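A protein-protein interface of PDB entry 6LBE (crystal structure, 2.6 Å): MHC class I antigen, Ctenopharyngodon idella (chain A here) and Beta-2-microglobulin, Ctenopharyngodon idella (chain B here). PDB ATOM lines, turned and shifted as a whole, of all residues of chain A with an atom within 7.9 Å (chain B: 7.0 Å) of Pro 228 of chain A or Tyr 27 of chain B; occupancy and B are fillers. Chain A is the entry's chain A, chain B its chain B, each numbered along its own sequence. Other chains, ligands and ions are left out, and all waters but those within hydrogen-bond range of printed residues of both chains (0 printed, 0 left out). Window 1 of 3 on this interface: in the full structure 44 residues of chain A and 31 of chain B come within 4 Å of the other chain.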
ATOM      1  N   THR A 199      11.446 -10.325  -2.660  1.00  0.00           N
ATOM      2  CA  THR A 199      10.473  -9.294  -2.326  1.00  0.00           C
ATOM      3  C   THR A 199       9.539  -9.792  -1.238  1.00  0.00           C
ATOM      4  O   THR A 199       9.317 -10.998  -1.094  1.00  0.00           O
ATOM      5  CB  THR A 199       9.626  -8.865  -3.535  1.00  0.00           C
ATOM      6  OG1 THR A 199       8.836  -7.723  -3.188  1.00  0.00           O
ATOM      7  CG2 THR A 199       8.693 -10.007  -4.002  1.00  0.00           C
ATOM      8  N   GLU A 225      19.854  -2.269  -5.338  1.00  0.00           N
ATOM      9  CA  GLU A 225      19.682  -1.576  -4.064  1.00  0.00           C
ATOM     10  C   GLU A 225      18.588  -2.238  -3.226  1.00  0.00           C
ATOM     11  O   GLU A 225      17.670  -2.879  -3.749  1.00  0.00           O
ATOM     12  CB  GLU A 225      19.285  -0.114  -4.294  1.00  0.00           C
ATOM     13  CG  GLU A 225      20.360   0.849  -4.827  1.00  0.00           C
ATOM     14  CD  GLU A 225      20.052   2.323  -4.508  1.00  0.00           C
ATOM     15  OE1 GLU A 225      21.002   3.104  -4.297  1.00  0.00           O
ATOM     16  OE2 GLU A 225      18.859   2.694  -4.429  1.00  0.00           O
ATOM     17  N   LEU A 226      18.663  -2.028  -1.913  1.00  0.00           N
ATOM     18  CA  LEU A 226      17.550  -2.347  -1.027  1.00  0.00           C
ATOM     19  C   LEU A 226      16.449  -1.306  -1.199  1.00  0.00           C
ATOM     20  O   LEU A 226      16.645  -0.113  -0.930  1.00  0.00           O
ATOM     21  CB  LEU A 226      18.017  -2.398   0.419  1.00  0.00           C
ATOM     22  CG  LEU A 226      16.985  -3.025   1.337  1.00  0.00           C
ATOM     23  CD1 LEU A 226      16.854  -4.518   1.060  1.00  0.00           C
ATOM     24  CD2 LEU A 226      17.397  -2.773   2.763  1.00  0.00           C
ATOM     25  N   LEU A 227      15.293  -1.754  -1.640  1.00  0.00           N
ATOM     26  CA  LEU A 227      14.185  -0.880  -1.961  1.00  0.00           C
ATOM     27  C   LEU A 227      13.014  -1.209  -1.055  1.00  0.00           C
ATOM     28  O   LEU A 227      12.932  -2.324  -0.535  1.00  0.00           O
ATOM     29  CB  LEU A 227      13.779  -1.055  -3.432  1.00  0.00           C
ATOM     30  CG  LEU A 227      14.816  -0.724  -4.509  1.00  0.00           C
ATOM     31  CD1 LEU A 227      14.312  -1.145  -5.876  1.00  0.00           C
ATOM     32  CD2 LEU A 227      15.145   0.771  -4.483  1.00  0.00           C
ATOM     33  N   PRO A 228      12.101  -0.270  -0.820  1.00  0.00           N
ATOM     34  CA  PRO A 228      10.890  -0.590  -0.056  1.00  0.00           C
ATOM     35  C   PRO A 228       9.698  -0.924  -0.941  1.00  0.00           C
ATOM     36  O   PRO A 228       9.615  -0.520  -2.092  1.00  0.00           O
ATOM     37  CB  PRO A 228      10.639   0.703   0.728  1.00  0.00           C
ATOM     38  CG  PRO A 228      11.114   1.755  -0.202  1.00  0.00           C
ATOM     39  CD  PRO A 228      12.296   1.183  -0.950  1.00  0.00           C
ATOM     40  N   ASN A 229       8.785  -1.712  -0.385  1.00  0.00           N
ATOM     41  CA  ASN A 229       7.460  -1.927  -0.952  1.00  0.00           C
ATOM     42  C   ASN A 229       6.465  -1.107  -0.136  1.00  0.00           C
ATOM     43  O   ASN A 229       6.835  -0.405   0.806  1.00  0.00           O
ATOM     44  CB  ASN A 229       6.990  -3.383  -0.809  1.00  0.00           C
ATOM     45  CG  ASN A 229       7.865  -4.361  -1.544  1.00  0.00           C
ATOM     46  OD1 ASN A 229       8.395  -4.061  -2.610  1.00  0.00           O
ATOM     47  ND2 ASN A 229       8.031  -5.543  -0.974  1.00  0.00           N
ATOM     48  N   GLU A 230       5.176  -1.229  -0.472  1.00  0.00           N
ATOM     49  CA  GLU A 230       4.119  -0.357   0.032  1.00  0.00           C
ATOM     50  C   GLU A 230       3.638  -0.731   1.434  1.00  0.00           C
ATOM     51  O   GLU A 230       2.975   0.084   2.094  1.00  0.00           O
ATOM     52  CB  GLU A 230       2.938  -0.384  -0.942  1.00  0.00           C
ATOM     53  CG  GLU A 230       1.998  -1.551  -0.758  1.00  0.00           C
ATOM     54  CD  GLU A 230       2.626  -2.892  -1.177  1.00  0.00           C
ATOM     55  OE1 GLU A 230       1.889  -3.911  -1.194  1.00  0.00           O
ATOM     56  OE2 GLU A 230       3.848  -2.931  -1.496  1.00  0.00           O
ATOM     57  N   ASP A 231       3.919  -1.946   1.882  1.00  0.00           N
ATOM     58  CA  ASP A 231       3.648  -2.418   3.234  1.00  0.00           C
ATOM     59  C   ASP A 231       4.977  -2.339   3.992  1.00  0.00           C
ATOM     60  O   ASP A 231       5.976  -1.857   3.450  1.00  0.00           O
ATOM     61  CB  ASP A 231       3.099  -3.851   3.149  1.00  0.00           C
ATOM     62  CG  ASP A 231       3.970  -4.753   2.280  1.00  0.00           C
ATOM     63  OD1 ASP A 231       5.210  -4.600   2.310  1.00  0.00           O
ATOM     64  OD2 ASP A 231       3.420  -5.655   1.603  1.00  0.00           O
ATOM     65  N   GLY A 232       5.022  -2.807   5.219  1.00  0.00           N
ATOM     66  CA  GLY A 232       6.320  -2.640   5.836  1.00  0.00           C
ATOM     67  C   GLY A 232       7.509  -3.357   5.227  1.00  0.00           C
ATOM     68  O   GLY A 232       8.632  -3.219   5.728  1.00  0.00           O
ATOM     69  N   SER A 233       7.310  -4.090   4.136  1.00  0.00           N
ATOM     70  CA  SER A 233       8.316  -5.016   3.636  1.00  0.00           C
ATOM     71  C   SER A 233       9.199  -4.360   2.573  1.00  0.00           C
ATOM     72  O   SER A 233       8.929  -3.256   2.083  1.00  0.00           O
ATOM     73  CB  SER A 233       7.658  -6.269   3.065  1.00  0.00           C
ATOM     74  OG  SER A 233       7.328  -6.063   1.713  1.00  0.00           O
ATOM     75  N   PHE A 234      10.262  -5.084   2.206  1.00  0.00           N
ATOM     76  CA  PHE A 234      11.321  -4.588   1.341  1.00  0.00           C
ATOM     77  C   PHE A 234      11.556  -5.578   0.212  1.00  0.00           C
ATOM     78  O   PHE A 234      11.065  -6.709   0.235  1.00  0.00           O
ATOM     79  CB  PHE A 234      12.613  -4.372   2.128  1.00  0.00           C
ATOM     80  CG  PHE A 234      12.467  -3.437   3.304  1.00  0.00           C
ATOM     81  CD1 PHE A 234      11.872  -3.867   4.487  1.00  0.00           C
ATOM     82  CD2 PHE A 234      12.961  -2.134   3.240  1.00  0.00           C
ATOM     83  CE1 PHE A 234      11.748  -3.005   5.566  1.00  0.00           C
ATOM     84  CE2 PHE A 234      12.857  -1.280   4.321  1.00  0.00           C
ATOM     85  CZ  PHE A 234      12.250  -1.710   5.479  1.00  0.00           C
ATOM     86  N   GLN A 235      12.316  -5.148  -0.788  1.00  0.00           N
ATOM     87  CA  GLN A 235      12.701  -6.019  -1.889  1.00  0.00           C
ATOM     88  C   GLN A 235      14.110  -5.658  -2.327  1.00  0.00           C
ATOM     89  O   GLN A 235      14.576  -4.537  -2.117  1.00  0.00           O
ATOM     90  CB  GLN A 235      11.755  -5.913  -3.097  1.00  0.00           C
ATOM     91  CG  GLN A 235      11.866  -4.614  -3.863  1.00  0.00           C
ATOM     92  CD  GLN A 235      11.049  -4.620  -5.137  1.00  0.00           C
ATOM     93  OE1 GLN A 235      11.593  -4.668  -6.243  1.00  0.00           O
ATOM     94  NE2 GLN A 235       9.733  -4.567  -4.994  1.00  0.00           N
ATOM     95  N   ARG A 236      14.788  -6.631  -2.935  1.00  0.00           N
ATOM     96  CA  ARG A 236      16.127  -6.430  -3.476  1.00  0.00           C
ATOM     97  C   ARG A 236      16.341  -7.479  -4.550  1.00  0.00           C
ATOM     98  O   ARG A 236      15.797  -8.579  -4.461  1.00  0.00           O
ATOM     99  CB  ARG A 236      17.197  -6.533  -2.387  1.00  0.00           C
ATOM    100  CG  ARG A 236      18.616  -6.302  -2.871  1.00  0.00           C
ATOM    101  CD  ARG A 236      19.572  -6.409  -1.711  1.00  0.00           C
ATOM    102  NE  ARG A 236      20.327  -5.178  -1.495  1.00  0.00           N
ATOM    103  CZ  ARG A 236      21.503  -5.124  -0.872  1.00  0.00           C
ATOM    104  NH1 ARG A 236      22.048  -6.223  -0.365  1.00  0.00           N
ATOM    105  NH2 ARG A 236      22.121  -3.970  -0.724  1.00  0.00           N
ATOM    106  N   LYS B   7      17.264  11.143  -7.770  1.00  0.00           N
ATOM    107  CA  LYS B   7      17.390   9.779  -8.272  1.00  0.00           C
ATOM    108  C   LYS B   7      16.018   9.119  -8.222  1.00  0.00           C
ATOM    109  O   LYS B   7      15.307   9.250  -7.227  1.00  0.00           O
ATOM    110  CB  LYS B   7      18.390   9.014  -7.416  1.00  0.00           C
ATOM    111  CG  LYS B   7      18.546   7.549  -7.723  1.00  0.00           C
ATOM    112  CD  LYS B   7      19.888   7.090  -7.175  1.00  0.00           C
ATOM    113  CE  LYS B   7      19.851   5.689  -6.607  1.00  0.00           C
ATOM    114  NZ  LYS B   7      20.972   5.588  -5.622  1.00  0.00           N
ATOM    115  N   VAL B   8      15.618   8.450  -9.299  1.00  0.00           N
ATOM    116  CA  VAL B   8      14.250   7.940  -9.405  1.00  0.00           C
ATOM    117  C   VAL B   8      14.275   6.476  -9.834  1.00  0.00           C
ATOM    118  O   VAL B   8      14.971   6.113 -10.788  1.00  0.00           O
ATOM    119  CB  VAL B   8      13.403   8.791 -10.373  1.00  0.00           C
ATOM    120  CG1 VAL B   8      12.117   8.102 -10.711  1.00  0.00           C
ATOM    121  CG2 VAL B   8      13.096  10.119  -9.732  1.00  0.00           C
ATOM    122  N   GLN B   9      13.525   5.636  -9.117  1.00  0.00           N
ATOM    123  CA  GLN B   9      13.476   4.202  -9.381  1.00  0.00           C
ATOM    124  C   GLN B   9      12.029   3.746  -9.436  1.00  0.00           C
ATOM    125  O   GLN B   9      11.299   3.887  -8.451  1.00  0.00           O
ATOM    126  CB  GLN B   9      14.243   3.424  -8.315  1.00  0.00           C
ATOM    127  CG  GLN B   9      15.738   3.534  -8.478  1.00  0.00           C
ATOM    128  CD  GLN B   9      16.503   2.989  -7.290  1.00  0.00           C
ATOM    129  OE1 GLN B   9      16.771   3.715  -6.323  1.00  0.00           O
ATOM    130  NE2 GLN B   9      16.882   1.726  -7.362  1.00  0.00           N
ATOM    131  N   VAL B  10      11.620   3.211 -10.586  1.00  0.00           N
ATOM    132  CA  VAL B  10      10.274   2.695 -10.813  1.00  0.00           C
ATOM    133  C   VAL B  10      10.345   1.176 -10.862  1.00  0.00           C
ATOM    134  O   VAL B  10      11.114   0.607 -11.647  1.00  0.00           O
ATOM    135  CB  VAL B  10       9.670   3.239 -12.121  1.00  0.00           C
ATOM    136  CG1 VAL B  10       8.147   3.136 -12.087  1.00  0.00           C
ATOM    137  CG2 VAL B  10      10.141   4.657 -12.400  1.00  0.00           C
ATOM    138  N   TYR B  11       9.530   0.521 -10.044  1.00  0.00           N
ATOM    139  CA  TYR B  11       9.497  -0.935 -10.000  1.00  0.00           C
ATOM    140  C   TYR B  11       8.132  -1.384  -9.504  1.00  0.00           C
ATOM    141  O   TYR B  11       7.322  -0.580  -9.027  1.00  0.00           O
ATOM    142  CB  TYR B  11      10.597  -1.499  -9.099  1.00  0.00           C
ATOM    143  CG  TYR B  11      10.674  -0.879  -7.718  1.00  0.00           C
ATOM    144  CD1 TYR B  11      11.358   0.315  -7.510  1.00  0.00           C
ATOM    145  CD2 TYR B  11      10.075  -1.487  -6.619  1.00  0.00           C
ATOM    146  CE1 TYR B  11      11.451   0.888  -6.245  1.00  0.00           C
ATOM    147  CE2 TYR B  11      10.151  -0.921  -5.346  1.00  0.00           C
ATOM    148  CZ  TYR B  11      10.849   0.266  -5.167  1.00  0.00           C
ATOM    149  OH  TYR B  11      10.956   0.830  -3.918  1.00  0.00           O
ATOM    150  N   ARG B  13       6.071  -4.267  -6.943  1.00  0.00           N
ATOM    151  CA  ARG B  13       6.304  -5.028  -5.720  1.00  0.00           C
ATOM    152  C   ARG B  13       6.679  -6.476  -6.043  1.00  0.00           C
ATOM    153  O   ARG B  13       7.712  -6.980  -5.594  1.00  0.00           O
ATOM    154  CB  ARG B  13       5.071  -4.980  -4.829  1.00  0.00           C
ATOM    155  CG  ARG B  13       5.190  -5.879  -3.632  1.00  0.00           C
ATOM    156  CD  ARG B  13       3.847  -6.145  -3.006  1.00  0.00           C
ATOM    157  NE  ARG B  13       3.965  -6.392  -1.574  1.00  0.00           N
ATOM    158  CZ  ARG B  13       4.437  -7.519  -1.052  1.00  0.00           C
ATOM    159  NH1 ARG B  13       4.828  -8.492  -1.857  1.00  0.00           N
ATOM    160  NH2 ARG B  13       4.515  -7.676   0.268  1.00  0.00           N
ATOM    161  N   ILE B  25       5.434   1.101  -7.865  1.00  0.00           N
ATOM    162  CA  ILE B  25       6.118   1.847  -6.807  1.00  0.00           C
ATOM    163  C   ILE B  25       7.164   2.781  -7.414  1.00  0.00           C
ATOM    164  O   ILE B  25       7.948   2.369  -8.277  1.00  0.00           O
ATOM    165  CB  ILE B  25       6.783   0.900  -5.791  1.00  0.00           C
ATOM    166  CG1 ILE B  25       5.737   0.021  -5.089  1.00  0.00           C
ATOM    167  CG2 ILE B  25       7.624   1.685  -4.800  1.00  0.00           C
ATOM    168  CD1 ILE B  25       6.321  -1.207  -4.453  1.00  0.00           C
ATOM    169  N   CYS B  26       7.176   4.037  -6.948  1.00  0.00           N
ATOM    170  CA  CYS B  26       8.167   5.048  -7.307  1.00  0.00           C
ATOM    171  C   CYS B  26       8.912   5.475  -6.045  1.00  0.00           C
ATOM    172  O   CYS B  26       8.308   6.040  -5.127  1.00  0.00           O
ATOM    173  CB  CYS B  26       7.512   6.266  -7.970  1.00  0.00           C
ATOM    174  SG  CYS B  26       8.692   7.221  -8.950  1.00  0.00           S
ATOM    175  N   TYR B  27      10.213   5.205  -5.996  1.00  0.00           N
ATOM    176  CA  TYR B  27      11.053   5.587  -4.869  1.00  0.00           C
ATOM    177  C   TYR B  27      12.001   6.683  -5.337  1.00  0.00           C
ATOM    178  O   TYR B  27      12.727   6.496  -6.315  1.00  0.00           O
ATOM    179  CB  TYR B  27      11.817   4.373  -4.332  1.00  0.00           C
ATOM    180  CG  TYR B  27      12.761   4.647  -3.177  1.00  0.00           C
ATOM    181  CD1 TYR B  27      12.272   4.928  -1.897  1.00  0.00           C
ATOM    182  CD2 TYR B  27      14.147   4.608  -3.356  1.00  0.00           C
ATOM    183  CE1 TYR B  27      13.136   5.179  -0.820  1.00  0.00           C
ATOM    184  CE2 TYR B  27      15.023   4.848  -2.276  1.00  0.00           C
ATOM    185  CZ  TYR B  27      14.509   5.133  -1.013  1.00  0.00           C
ATOM    186  OH  TYR B  27      15.368   5.383   0.046  1.00  0.00           O
ATOM    187  N   VAL B  28      11.982   7.825  -4.648  1.00  0.00           N
ATOM    188  CA  VAL B  28      12.665   9.039  -5.089  1.00  0.00           C
ATOM    189  C   VAL B  28      13.560   9.496  -3.956  1.00  0.00           C
ATOM    190  O   VAL B  28      13.104   9.624  -2.818  1.00  0.00           O
ATOM    191  CB  VAL B  28      11.669  10.158  -5.472  1.00  0.00           C
ATOM    192  CG1 VAL B  28      12.405  11.417  -5.907  1.00  0.00           C
ATOM    193  CG2 VAL B  28      10.729   9.698  -6.561  1.00  0.00           C
ATOM    194  N   SER B  29      14.823   9.760  -4.252  1.00  0.00           N
ATOM    195  CA  SER B  29      15.749   9.982  -3.154  1.00  0.00           C
ATOM    196  C   SER B  29      16.900  10.848  -3.615  1.00  0.00           C
ATOM    197  O   SER B  29      17.159  10.989  -4.814  1.00  0.00           O
ATOM    198  CB  SER B  29      16.289   8.665  -2.604  1.00  0.00           C
ATOM    199  OG  SER B  29      16.990   8.013  -3.639  1.00  0.00           O
ATOM    200  N   GLY B  30      17.589  11.426  -2.626  1.00  0.00           N
ATOM    201  CA  GLY B  30      18.768  12.242  -2.856  1.00  0.00           C
ATOM    202  C   GLY B  30      18.502  13.578  -3.505  1.00  0.00           C
ATOM    203  O   GLY B  30      19.402  14.135  -4.130  1.00  0.00           O
ATOM    204  N   ILE B  38       5.420  13.991  -7.262  1.00  0.00           N
ATOM    205  CA  ILE B  38       5.530  12.666  -7.858  1.00  0.00           C
ATOM    206  C   ILE B  38       4.160  12.196  -8.318  1.00  0.00           C
ATOM    207  O   ILE B  38       3.202  12.211  -7.542  1.00  0.00           O
ATOM    208  CB  ILE B  38       6.121  11.654  -6.863  1.00  0.00           C
ATOM    209  CG1 ILE B  38       7.445  12.174  -6.279  1.00  0.00           C
ATOM    210  CG2 ILE B  38       6.270  10.285  -7.519  1.00  0.00           C
ATOM    211  CD1 ILE B  38       7.890  11.423  -5.006  1.00  0.00           C
ATOM    212  N   THR B  53       4.304   8.520   0.856  1.00  0.00           N
ATOM    213  CA  THR B  53       4.804   8.515   2.216  1.00  0.00           C
ATOM    214  C   THR B  53       5.130   9.938   2.663  1.00  0.00           C
ATOM    215  O   THR B  53       5.244  10.863   1.856  1.00  0.00           O
ATOM    216  CB  THR B  53       6.029   7.604   2.325  1.00  0.00           C
ATOM    217  OG1 THR B  53       7.076   8.076   1.462  1.00  0.00           O
ATOM    218  CG2 THR B  53       5.651   6.212   1.921  1.00  0.00           C
ATOM    219  N   GLU B  58      17.193   9.561   6.116  1.00  0.00           N
ATOM    220  CA  GLU B  58      18.062   8.674   6.867  1.00  0.00           C
ATOM    221  C   GLU B  58      19.371   9.410   7.170  1.00  0.00           C
ATOM    222  O   GLU B  58      19.537  10.594   6.842  1.00  0.00           O
ATOM    223  CB  GLU B  58      18.368   7.448   6.018  1.00  0.00           C
ATOM    224  CG  GLU B  58      18.531   7.762   4.533  1.00  0.00           C
ATOM    225  CD  GLU B  58      18.485   6.499   3.655  1.00  0.00           C
ATOM    226  OE1 GLU B  58      17.898   5.483   4.105  1.00  0.00           O
ATOM    227  OE2 GLU B  58      19.044   6.518   2.526  1.00  0.00           O
ATOM    228  N   GLN B  62      19.951  12.399   3.381  1.00  0.00           N
ATOM    229  CA  GLN B  62      19.322  12.298   2.067  1.00  0.00           C
ATOM    230  C   GLN B  62      17.818  12.090   2.219  1.00  0.00           C
ATOM    231  O   GLN B  62      17.369  11.157   2.908  1.00  0.00           O
ATOM    232  CB  GLN B  62      19.938  11.151   1.262  1.00  0.00           C
ATOM    233  CG  GLN B  62      21.424  11.349   0.938  1.00  0.00           C
ATOM    234  CD  GLN B  62      21.667  12.057  -0.374  1.00  0.00           C
ATOM    235  OE1 GLN B  62      21.786  11.417  -1.420  1.00  0.00           O
ATOM    236  NE2 GLN B  62      21.766  13.387  -0.328  1.00  0.00           N
ATOM    237  N   PHE B  63      17.044  12.965   1.573  1.00  0.00           N
ATOM    238  CA  PHE B  63      15.592  12.829   1.581  1.00  0.00           C
ATOM    239  C   PHE B  63      15.160  11.647   0.735  1.00  0.00           C
ATOM    240  O   PHE B  63      15.832  11.264  -0.218  1.00  0.00           O
ATOM    241  CB  PHE B  63      14.933  14.095   1.061  1.00  0.00           C
ATOM    242  CG  PHE B  63      15.057  15.256   2.000  1.00  0.00           C
ATOM    243  CD1 PHE B  63      14.318  15.287   3.172  1.00  0.00           C
ATOM    244  CD2 PHE B  63      15.930  16.316   1.714  1.00  0.00           C
ATOM    245  CE1 PHE B  63      14.436  16.352   4.042  1.00  0.00           C
ATOM    246  CE2 PHE B  63      16.058  17.375   2.574  1.00  0.00           C
ATOM    247  CZ  PHE B  63      15.304  17.400   3.743  1.00  0.00           C
ATOM    248  N   HIS B  64      14.041  11.046   1.101  1.00  0.00           N
ATOM    249  CA  HIS B  64      13.501   9.973   0.285  1.00  0.00           C
ATOM    250  C   HIS B  64      11.989   9.981   0.410  1.00  0.00           C
ATOM    251  O   HIS B  64      11.433  10.345   1.450  1.00  0.00           O
ATOM    252  CB  HIS B  64      14.074   8.598   0.655  1.00  0.00           C
ATOM    253  CG  HIS B  64      13.847   8.185   2.081  1.00  0.00           C
ATOM    254  ND1 HIS B  64      12.596   7.925   2.601  1.00  0.00           N
ATOM    255  CD2 HIS B  64      14.722   7.952   3.085  1.00  0.00           C
ATOM    256  CE1 HIS B  64      12.707   7.570   3.867  1.00  0.00           C
ATOM    257  NE2 HIS B  64      13.988   7.575   4.185  1.00  0.00           N
ATOM    258  N   LEU B  65      11.332   9.578  -0.669  1.00  0.00           N
ATOM    259  CA  LEU B  65       9.884   9.573  -0.738  1.00  0.00           C
ATOM    260  C   LEU B  65       9.470   8.396  -1.599  1.00  0.00           C
ATOM    261  O   LEU B  65      10.201   8.000  -2.509  1.00  0.00           O
ATOM    262  CB  LEU B  65       9.349  10.889  -1.320  1.00  0.00           C
ATOM    263  CG  LEU B  65       9.161  12.079  -0.379  1.00  0.00           C
ATOM    264  CD1 LEU B  65       8.990  13.371  -1.172  1.00  0.00           C
ATOM    265  CD2 LEU B  65       7.974  11.869   0.549  1.00  0.00           C
ATOM    266  N   THR B  66       8.300   7.836  -1.306  1.00  0.00           N
ATOM    267  CA  THR B  66       7.748   6.735  -2.085  1.00  0.00           C
ATOM    268  C   THR B  66       6.331   7.077  -2.512  1.00  0.00           C
ATOM    269  O   THR B  66       5.585   7.712  -1.760  1.00  0.00           O
ATOM    270  CB  THR B  66       7.720   5.401  -1.287  1.00  0.00           C
ATOM    271  OG1 THR B  66       9.030   5.066  -0.807  1.00  0.00           O
ATOM    272  CG2 THR B  66       7.212   4.270  -2.163  1.00  0.00           C
ATOM    273  N   LYS B  67       5.957   6.665  -3.711  1.00  0.00           N
ATOM    274  CA  LYS B  67       4.557   6.651  -4.111  1.00  0.00           C
ATOM    275  C   LYS B  67       4.247   5.302  -4.739  1.00  0.00           C
ATOM    276  O   LYS B  67       5.063   4.752  -5.480  1.00  0.00           O
ATOM    277  CB  LYS B  67       4.204   7.781  -5.096  1.00  0.00           C
ATOM    278  CG  LYS B  67       2.787   7.665  -5.662  1.00  0.00           C
ATOM    279  CD  LYS B  67       2.299   8.929  -6.342  1.00  0.00           C
ATOM    280  CE  LYS B  67       2.266  10.078  -5.396  1.00  0.00           C
ATOM    281  NZ  LYS B  67       1.417  11.161  -5.957  1.00  0.00           N
ATOM    282  N   CYS B  81       6.467   7.018 -13.995  1.00  0.00           N
ATOM    283  CA  CYS B  81       6.594   7.887 -12.852  1.00  0.00           C
ATOM    284  C   CYS B  81       7.111   9.220 -13.363  1.00  0.00           C
ATOM    285  O   CYS B  81       8.117   9.255 -14.078  1.00  0.00           O
ATOM    286  CB  CYS B  81       7.541   7.288 -11.817  1.00  0.00           C
ATOM    287  SG  CYS B  81       7.651   8.302 -10.356  1.00  0.00           S
ATOM    288  N   VAL B  83       8.347  13.047 -12.186  1.00  0.00           N
ATOM    289  CA  VAL B  83       8.916  13.737 -11.034  1.00  0.00           C
ATOM    290  C   VAL B  83       9.208  15.189 -11.401  1.00  0.00           C
ATOM    291  O   VAL B  83       9.807  15.472 -12.446  1.00  0.00           O
ATOM    292  CB  VAL B  83      10.194  13.030 -10.544  1.00  0.00           C
ATOM    293  CG1 VAL B  83      10.928  13.896  -9.526  1.00  0.00           C
ATOM    294  CG2 VAL B  83       9.846  11.695  -9.929  1.00  0.00           C
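The side-chain amino group (NZ) of Lys 7 of chain B is in salt-bridge range of the side-chain carboxylate (OE1) of Glu 225 of chain A, 2.8 Å away.
NH2 of Arg 13 of chain B lies within salt-bridge range of OD2 of Asp 231 of chain A, 2.7 Å away.
The backbone carbonyl oxygen (O) of Arg 13 of chain B lies within hydrogen-bond range of the side-chain hydroxyl (OG1) of Thr 199 of chain A, at 2.8 Å.
The side-chain carboxylate (OE2) of Glu 225 of chain A sits close to the side-chain amide oxygen (OE1) of Gln 9 of chain B (3.0 Å).
The side-chain carboxylate (OE1) of Glu 230 of chain A lies within salt-bridge range of the guanidinium group (NE) of Arg 13 of chain B (3.3 Å).
O of Pro 228 of chain A lies within hydrogen-bond range of OH of Tyr 11 of chain B (2.6 Å).
The side-chain amide nitrogen (NE2) of Gln 235 of chain A is in hydrogen-bond range of the backbone carbonyl oxygen (O) of Arg 13 of chain B (3.2 Å).
OD1 of Asp 231 of chain A lies within hydrogen-bond range of OG of Ser 233 of chain A, at 2.6 Å.
The backbone carbonyl oxygen (O) of Phe 234 of chain A lies within hydrogen-bond range of the side-chain amide nitrogen (ND2) of Asn 229 of chain A (3.5 Å).
The side-chain amide nitrogen of Asn 229 of chain A sits at hydrogen-bond distance from the side-chain hydroxyl of Ser 233 of chain A (2.8 Å).
The backbone NH (N) of Thr 53 of chain B is in hydrogen-bond range of the backbone carbonyl oxygen (O) of Thr 66 of chain B (3.0 Å).
O of Gln 9 of chain B lies within hydrogen-bond range of N of Tyr 27 of chain B.
The side-chain amide nitrogen of Gln 235 of chain A is in hydrogen-bond range of the side-chain amide oxygen of Asn 229 of chain A, 2.8 Å away.
Leu 227 of chain A touches Gln 9 of chain B.
Leu 227 of chain A touches Tyr 11 of chain B.
CG of Pro 228 of chain A touches CD1 of Tyr 27 of chain B (3.8 Å).
Pro 228 of chain A touches Thr 66 of chain B (CG to OG1, 3.96 Å).
CG of Arg 13 of chain B touches CG of Asn 229 of chain A, at 3.7 Å.
Ile 25 of chain B touches Asn 229 of chain A (CD1 to CA, 3.8 Å).
OG of Ser 233 of chain A touches NH2 of Arg 13 of chain B, at 3.6 Å.
Tyr 11 of chain B touches Gln 235 of chain A.
Of the printed residues of chain B, Thr 199 of chain A touches Arg 13 (2.8 Å).
Printed residues of chain B within 4 Å of Glu 225 of chain A: Lys 7 and Gln 9.
Printed residues of chain B within 4 Å of Asp 231 of chain A: Arg 13 (2.7 Å).
Of the printed residues of chain A, Lys 7 of chain B touches Glu 225 (2.8 Å).
Of the printed residues of chain A, Gln 9 of chain B touches Glu 225 (3.0 Å) and Leu 227 (3.5 Å).
Tyr 27 of chain B touches one residue of chain A.
The nearest printed residue of chain B that does not touch Pro 228 of chain A is Ile 25 of chain B (4.02 Å).
The nearest residue of chain A that does not touch Tyr 27 of chain B is Leu 227 of chain A (4.1 Å).
Of the 23 printed residues of chain B, 7 touch a printed residue of chain A.
Hydrophobic or aromatic side chains of chain B that line the printed part of chain A: Tyr 11, Ile 25 and Tyr 27.
Of the 13 printed residues of chain A, 9 touch a printed residue of chain B.
Hydrophobic or aromatic side chains of chain A within 4 Å of the printed part of chain B: Leu 227 and Pro 228.
Among the printed residues, 15 pairs touch across the chains.
Among the printed residues, Asp or Glu carboxylates within 4 Å of a Lys or Arg side-chain nitrogen of the other chain: Glu 225 of chain A with Lys 7 of chain B (2.8 Å), Glu 230 of chain A with Arg 13 of chain B (3.3 Å) and Asp 231 of chain A with Arg 13 of chain B (2.7 Å).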
